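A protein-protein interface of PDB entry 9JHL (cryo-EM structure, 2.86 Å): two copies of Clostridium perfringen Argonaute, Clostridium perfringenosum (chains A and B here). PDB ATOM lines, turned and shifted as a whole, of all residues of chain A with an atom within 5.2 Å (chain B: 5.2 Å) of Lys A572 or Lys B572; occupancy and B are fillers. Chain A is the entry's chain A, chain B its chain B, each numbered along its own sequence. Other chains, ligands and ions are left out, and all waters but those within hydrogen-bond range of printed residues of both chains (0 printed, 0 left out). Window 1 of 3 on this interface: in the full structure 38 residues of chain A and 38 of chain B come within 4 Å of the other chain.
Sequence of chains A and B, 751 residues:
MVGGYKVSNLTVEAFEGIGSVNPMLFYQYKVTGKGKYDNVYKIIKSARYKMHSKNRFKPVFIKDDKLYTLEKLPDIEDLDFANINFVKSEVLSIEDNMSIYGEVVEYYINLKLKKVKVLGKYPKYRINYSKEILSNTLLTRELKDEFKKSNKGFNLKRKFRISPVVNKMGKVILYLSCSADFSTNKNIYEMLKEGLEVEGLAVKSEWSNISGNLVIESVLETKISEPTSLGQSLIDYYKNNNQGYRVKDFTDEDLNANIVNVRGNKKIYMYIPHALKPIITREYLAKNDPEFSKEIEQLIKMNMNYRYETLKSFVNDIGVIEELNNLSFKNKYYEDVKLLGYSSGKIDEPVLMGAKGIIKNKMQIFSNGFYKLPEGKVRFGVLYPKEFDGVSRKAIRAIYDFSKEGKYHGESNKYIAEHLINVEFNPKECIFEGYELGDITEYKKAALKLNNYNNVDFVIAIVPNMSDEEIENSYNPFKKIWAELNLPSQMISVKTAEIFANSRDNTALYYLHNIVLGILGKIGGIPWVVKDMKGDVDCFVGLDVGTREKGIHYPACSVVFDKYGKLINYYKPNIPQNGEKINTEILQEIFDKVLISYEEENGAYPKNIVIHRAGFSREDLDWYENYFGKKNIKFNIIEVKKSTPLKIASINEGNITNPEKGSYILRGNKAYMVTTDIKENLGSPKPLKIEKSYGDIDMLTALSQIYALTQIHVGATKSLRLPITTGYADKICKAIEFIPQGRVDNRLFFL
Of the 10 printed residues of chain A, 3 touch a printed residue of chain B. Among the printed residues, no Asp or Glu carboxylate lies within 4 Å of a Lys or Arg side-chain nitrogen of the other chain.
Lys A572 touches just one residue of chain B: Lys B572. Lys B572 touches one residue of chain A. Printed residues of chain B within 4 Å of Ile A736: Asn B574. Of the printed residues of chain A, Asn B574 touches Ile A736. Of the printed residues of chain B, Asn A574 touches Ile B736 (3.3 Å). Tyr B570 touches none of the printed residues of chain A. Ile B739 touches none of the printed residues of chain A.
NZ of Lys A572 sits at hydrogen-bond distance from OD1 of Asn A574 (3.5 Å). NZ of Lys B572 sits at hydrogen-bond distance from OD1 of Asn B574 (3.5 Å).
Lys B572 touches Lys A572. O of Ile B736 touches CB of Asn A574, at 3.3 Å. CB of Asn B574 touches O of Ile A736, 3.4 Å away.
Lys B572 touches its own counterpart, Lys A572. Asn A574 touches Ile B736, and with the chains exchanged Ile A736 touches Asn B574. Positions printed for both chains: 555, 556, 557, 570, 571, 572, 573, 574, 736 and 739. Of the 3 pairs that touch across the chains among the printed residues, 3 have their exchanged pair printed and touching as well.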
ATOM      1  N   PRO A 555       8.278  -0.982 -25.385  1.00  0.00           N
ATOM      2  CA  PRO A 555       7.141  -1.806 -25.809  1.00  0.00           C
ATOM      3  C   PRO A 555       6.103  -1.958 -24.707  1.00  0.00           C
ATOM      4  O   PRO A 555       6.398  -1.819 -23.521  1.00  0.00           O
ATOM      5  CB  PRO A 555       7.792  -3.146 -26.159  1.00  0.00           C
ATOM      6  CG  PRO A 555       9.177  -2.780 -26.560  1.00  0.00           C
ATOM      7  CD  PRO A 555       9.564  -1.648 -25.658  1.00  0.00           C
ATOM      8  N   ALA A 556       4.869  -2.231 -25.125  1.00  0.00           N
ATOM      9  CA  ALA A 556       3.720  -2.266 -24.224  1.00  0.00           C
ATOM     10  C   ALA A 556       3.784  -3.527 -23.377  1.00  0.00           C
ATOM     11  O   ALA A 556       3.106  -4.519 -23.648  1.00  0.00           O
ATOM     12  CB  ALA A 556       2.424  -2.209 -25.019  1.00  0.00           C
ATOM     13  N   CYS A 557       4.594  -3.478 -22.326  1.00  0.00           N
ATOM     14  CA  CYS A 557       4.828  -4.643 -21.489  1.00  0.00           C
ATOM     15  C   CYS A 557       3.610  -4.978 -20.643  1.00  0.00           C
ATOM     16  O   CYS A 557       2.968  -4.091 -20.077  1.00  0.00           O
ATOM     17  CB  CYS A 557       6.025  -4.416 -20.575  1.00  0.00           C
ATOM     18  SG  CYS A 557       6.303  -5.811 -19.490  1.00  0.00           S
ATOM     19  N   TYR A 570       4.833 -12.978 -18.764  1.00  0.00           N
ATOM     20  CA  TYR A 570       5.010 -11.605 -19.208  1.00  0.00           C
ATOM     21  C   TYR A 570       5.071 -11.601 -20.728  1.00  0.00           C
ATOM     22  O   TYR A 570       5.546 -12.563 -21.335  1.00  0.00           O
ATOM     23  CB  TYR A 570       6.271 -10.952 -18.611  1.00  0.00           C
ATOM     24  CG  TYR A 570       7.596 -11.552 -19.033  1.00  0.00           C
ATOM     25  CD1 TYR A 570       8.166 -12.591 -18.311  1.00  0.00           C
ATOM     26  CD2 TYR A 570       8.298 -11.053 -20.129  1.00  0.00           C
ATOM     27  CE1 TYR A 570       9.377 -13.134 -18.682  1.00  0.00           C
ATOM     28  CE2 TYR A 570       9.500 -11.596 -20.512  1.00  0.00           C
ATOM     29  CZ  TYR A 570      10.033 -12.640 -19.789  1.00  0.00           C
ATOM     30  OH  TYR A 570      11.242 -13.179 -20.161  1.00  0.00           O
ATOM     31  N   TYR A 571       4.595 -10.525 -21.344  1.00  0.00           N
ATOM     32  CA  TYR A 571       4.587 -10.419 -22.796  1.00  0.00           C
ATOM     33  C   TYR A 571       5.147  -9.072 -23.213  1.00  0.00           C
ATOM     34  O   TYR A 571       4.521  -8.036 -22.980  1.00  0.00           O
ATOM     35  CB  TYR A 571       3.179 -10.603 -23.363  1.00  0.00           C
ATOM     36  CG  TYR A 571       3.145 -10.566 -24.872  1.00  0.00           C
ATOM     37  CD1 TYR A 571       3.615 -11.635 -25.619  1.00  0.00           C
ATOM     38  CD2 TYR A 571       2.654  -9.461 -25.548  1.00  0.00           C
ATOM     39  CE1 TYR A 571       3.594 -11.607 -26.994  1.00  0.00           C
ATOM     40  CE2 TYR A 571       2.628  -9.423 -26.922  1.00  0.00           C
ATOM     41  CZ  TYR A 571       3.099 -10.498 -27.640  1.00  0.00           C
ATOM     42  OH  TYR A 571       3.074 -10.467 -29.015  1.00  0.00           O
ATOM     43  N   LYS A 572       6.314  -9.095 -23.844  1.00  0.00           N
ATOM     44  CA  LYS A 572       6.900  -7.918 -24.474  1.00  0.00           C
ATOM     45  C   LYS A 572       6.605  -7.995 -25.963  1.00  0.00           C
ATOM     46  O   LYS A 572       7.081  -8.927 -26.634  1.00  0.00           O
ATOM     47  CB  LYS A 572       8.409  -7.865 -24.218  1.00  0.00           C
ATOM     48  CG  LYS A 572       9.146  -6.636 -24.743  1.00  0.00           C
ATOM     49  CD  LYS A 572       9.840  -6.865 -26.085  1.00  0.00           C
ATOM     50  CE  LYS A 572      10.993  -7.833 -25.982  1.00  0.00           C
ATOM     51  NZ  LYS A 572      11.664  -8.047 -27.291  1.00  0.00           N
ATOM     52  N   PRO A 573       5.816  -7.080 -26.520  1.00  0.00           N
ATOM     53  CA  PRO A 573       5.648  -7.040 -27.975  1.00  0.00           C
ATOM     54  C   PRO A 573       6.931  -6.601 -28.660  1.00  0.00           C
ATOM     55  O   PRO A 573       7.624  -5.696 -28.197  1.00  0.00           O
ATOM     56  CB  PRO A 573       4.527  -6.016 -28.172  1.00  0.00           C
ATOM     57  CG  PRO A 573       3.802  -6.011 -26.883  1.00  0.00           C
ATOM     58  CD  PRO A 573       4.839  -6.223 -25.836  1.00  0.00           C
ATOM     59  N   ASN A 574       7.234  -7.245 -29.785  1.00  0.00           N
ATOM     60  CA  ASN A 574       8.522  -7.033 -30.437  1.00  0.00           C
ATOM     61  C   ASN A 574       8.572  -5.689 -31.149  1.00  0.00           C
ATOM     62  O   ASN A 574       9.658  -5.172 -31.435  1.00  0.00           O
ATOM     63  CB  ASN A 574       8.794  -8.172 -31.414  1.00  0.00           C
ATOM     64  CG  ASN A 574       8.994  -9.494 -30.715  1.00  0.00           C
ATOM     65  OD1 ASN A 574       9.677  -9.573 -29.696  1.00  0.00           O
ATOM     66  ND2 ASN A 574       8.384 -10.544 -31.249  1.00  0.00           N
ATOM     67  N   ILE A 736      14.688  -4.120 -20.289  1.00  0.00           N
ATOM     68  CA  ILE A 736      14.065  -4.414 -21.575  1.00  0.00           C
ATOM     69  C   ILE A 736      15.087  -4.909 -22.587  1.00  0.00           C
ATOM     70  O   ILE A 736      14.733  -5.658 -23.506  1.00  0.00           O
ATOM     71  CB  ILE A 736      13.298  -3.162 -22.045  1.00  0.00           C
ATOM     72  CG1 ILE A 736      12.338  -3.470 -23.192  1.00  0.00           C
ATOM     73  CG2 ILE A 736      14.227  -2.017 -22.365  1.00  0.00           C
ATOM     74  CD1 ILE A 736      11.134  -4.233 -22.754  1.00  0.00           C
ATOM     75  N   ILE A 739      16.005  -9.009 -21.472  1.00  0.00           N
ATOM     76  CA  ILE A 739      15.007 -10.080 -21.518  1.00  0.00           C
ATOM     77  C   ILE A 739      15.655 -11.333 -22.091  1.00  0.00           C
ATOM     78  O   ILE A 739      16.293 -11.257 -23.157  1.00  0.00           O
ATOM     79  CB  ILE A 739      13.800  -9.642 -22.353  1.00  0.00           C
ATOM     80  CG1 ILE A 739      13.138  -8.436 -21.697  1.00  0.00           C
ATOM     81  CG2 ILE A 739      12.798 -10.766 -22.506  1.00  0.00           C
ATOM     82  CD1 ILE A 739      12.033  -7.844 -22.472  1.00  0.00           C
ATOM     83  N   PRO B 555      13.846  -1.574 -34.888  1.00  0.00           N
ATOM     84  CA  PRO B 555      15.184  -1.621 -34.291  1.00  0.00           C
ATOM     85  C   PRO B 555      16.276  -1.706 -35.346  1.00  0.00           C
ATOM     86  O   PRO B 555      16.051  -2.148 -36.473  1.00  0.00           O
ATOM     87  CB  PRO B 555      15.137  -2.881 -33.424  1.00  0.00           C
ATOM     88  CG  PRO B 555      13.699  -3.019 -33.068  1.00  0.00           C
ATOM     89  CD  PRO B 555      12.945  -2.572 -34.283  1.00  0.00           C
ATOM     90  N   ALA B 556      17.470  -1.258 -34.966  1.00  0.00           N
ATOM     91  CA  ALA B 556      18.596  -1.127 -35.886  1.00  0.00           C
ATOM     92  C   ALA B 556      19.145  -2.508 -36.208  1.00  0.00           C
ATOM     93  O   ALA B 556      20.154  -2.945 -35.654  1.00  0.00           O
ATOM     94  CB  ALA B 556      19.675  -0.241 -35.278  1.00  0.00           C
ATOM     95  N   CYS B 557      18.481  -3.193 -37.133  1.00  0.00           N
ATOM     96  CA  CYS B 557      18.834  -4.563 -37.467  1.00  0.00           C
ATOM     97  C   CYS B 557      20.146  -4.631 -38.233  1.00  0.00           C
ATOM     98  O   CYS B 557      20.396  -3.830 -39.135  1.00  0.00           O
ATOM     99  CB  CYS B 557      17.735  -5.214 -38.295  1.00  0.00           C
ATOM    100  SG  CYS B 557      18.169  -6.883 -38.773  1.00  0.00           S
ATOM    101  N   TYR B 570      22.596 -12.468 -36.970  1.00  0.00           N
ATOM    102  CA  TYR B 570      21.816 -11.243 -37.041  1.00  0.00           C
ATOM    103  C   TYR B 570      21.632 -10.714 -35.627  1.00  0.00           C
ATOM    104  O   TYR B 570      21.561 -11.492 -34.673  1.00  0.00           O
ATOM    105  CB  TYR B 570      20.451 -11.452 -37.724  1.00  0.00           C
ATOM    106  CG  TYR B 570      19.476 -12.360 -37.002  1.00  0.00           C
ATOM    107  CD1 TYR B 570      19.463 -13.725 -37.247  1.00  0.00           C
ATOM    108  CD2 TYR B 570      18.541 -11.845 -36.107  1.00  0.00           C
ATOM    109  CE1 TYR B 570      18.571 -14.556 -36.603  1.00  0.00           C
ATOM    110  CE2 TYR B 570      17.656 -12.667 -35.452  1.00  0.00           C
ATOM    111  CZ  TYR B 570      17.677 -14.021 -35.699  1.00  0.00           C
ATOM    112  OH  TYR B 570      16.786 -14.847 -35.056  1.00  0.00           O
ATOM    113  N   TYR B 571      21.552  -9.396 -35.485  1.00  0.00           N
ATOM    114  CA  TYR B 571      21.395  -8.776 -34.178  1.00  0.00           C
ATOM    115  C   TYR B 571      20.282  -7.746 -34.231  1.00  0.00           C
ATOM    116  O   TYR B 571      20.428  -6.704 -34.877  1.00  0.00           O
ATOM    117  CB  TYR B 571      22.695  -8.126 -33.705  1.00  0.00           C
ATOM    118  CG  TYR B 571      22.583  -7.532 -32.320  1.00  0.00           C
ATOM    119  CD1 TYR B 571      22.552  -8.348 -31.199  1.00  0.00           C
ATOM    120  CD2 TYR B 571      22.501  -6.162 -32.135  1.00  0.00           C
ATOM    121  CE1 TYR B 571      22.443  -7.815 -29.935  1.00  0.00           C
ATOM    122  CE2 TYR B 571      22.392  -5.620 -30.876  1.00  0.00           C
ATOM    123  CZ  TYR B 571      22.365  -6.451 -29.780  1.00  0.00           C
ATOM    124  OH  TYR B 571      22.259  -5.916 -28.519  1.00  0.00           O
ATOM    125  N   LYS B 572      19.188  -8.030 -33.539  1.00  0.00           N
ATOM    126  CA  LYS B 572      18.107  -7.074 -33.332  1.00  0.00           C
ATOM    127  C   LYS B 572      18.281  -6.471 -31.946  1.00  0.00           C
ATOM    128  O   LYS B 572      18.191  -7.203 -30.945  1.00  0.00           O
ATOM    129  CB  LYS B 572      16.746  -7.762 -33.460  1.00  0.00           C
ATOM    130  CG  LYS B 572      15.516  -6.864 -33.357  1.00  0.00           C
ATOM    131  CD  LYS B 572      14.874  -6.861 -31.969  1.00  0.00           C
ATOM    132  CE  LYS B 572      14.254  -8.191 -31.616  1.00  0.00           C
ATOM    133  NZ  LYS B 572      13.632  -8.179 -30.267  1.00  0.00           N
ATOM    134  N   PRO B 573      18.558  -5.175 -31.830  1.00  0.00           N
ATOM    135  CA  PRO B 573      18.571  -4.542 -30.507  1.00  0.00           C
ATOM    136  C   PRO B 573      17.170  -4.474 -29.924  1.00  0.00           C
ATOM    137  O   PRO B 573      16.200  -4.185 -30.622  1.00  0.00           O
ATOM    138  CB  PRO B 573      19.131  -3.146 -30.792  1.00  0.00           C
ATOM    139  CG  PRO B 573      19.890  -3.301 -32.052  1.00  0.00           C
ATOM    140  CD  PRO B 573      19.133  -4.299 -32.859  1.00  0.00           C
ATOM    141  N   ASN B 574      17.077  -4.728 -28.619  1.00  0.00           N
ATOM    142  CA  ASN B 574      15.772  -4.861 -27.983  1.00  0.00           C
ATOM    143  C   ASN B 574      15.095  -3.509 -27.805  1.00  0.00           C
ATOM    144  O   ASN B 574      13.873  -3.436 -27.636  1.00  0.00           O
ATOM    145  CB  ASN B 574      15.928  -5.565 -26.640  1.00  0.00           C
ATOM    146  CG  ASN B 574      16.367  -7.002 -26.791  1.00  0.00           C
ATOM    147  OD1 ASN B 574      15.869  -7.727 -27.650  1.00  0.00           O
ATOM    148  ND2 ASN B 574      17.318  -7.420 -25.966  1.00  0.00           N
ATOM    149  N   ILE B 736       9.824  -8.747 -37.932  1.00  0.00           N
ATOM    150  CA  ILE B 736      10.402  -8.258 -36.686  1.00  0.00           C
ATOM    151  C   ILE B 736       9.607  -8.736 -35.480  1.00  0.00           C
ATOM    152  O   ILE B 736      10.167  -8.873 -34.386  1.00  0.00           O
ATOM    153  CB  ILE B 736      10.524  -6.724 -36.770  1.00  0.00           C
ATOM    154  CG1 ILE B 736      11.423  -6.156 -35.674  1.00  0.00           C
ATOM    155  CG2 ILE B 736       9.174  -6.052 -36.809  1.00  0.00           C
ATOM    156  CD1 ILE B 736      12.871  -6.437 -35.907  1.00  0.00           C
ATOM    157  N   ILE B 739      10.612 -12.931 -34.949  1.00  0.00           N
ATOM    158  CA  ILE B 739      11.962 -13.379 -34.602  1.00  0.00           C
ATOM    159  C   ILE B 739      11.861 -14.485 -33.560  1.00  0.00           C
ATOM    160  O   ILE B 739      11.166 -14.306 -32.545  1.00  0.00           O
ATOM    161  CB  ILE B 739      12.795 -12.202 -34.089  1.00  0.00           C
ATOM    162  CG1 ILE B 739      12.934 -11.158 -35.191  1.00  0.00           C
ATOM    163  CG2 ILE B 739      14.164 -12.653 -33.623  1.00  0.00           C
ATOM    164  CD1 ILE B 739      13.615  -9.917 -34.781  1.00  0.00           C
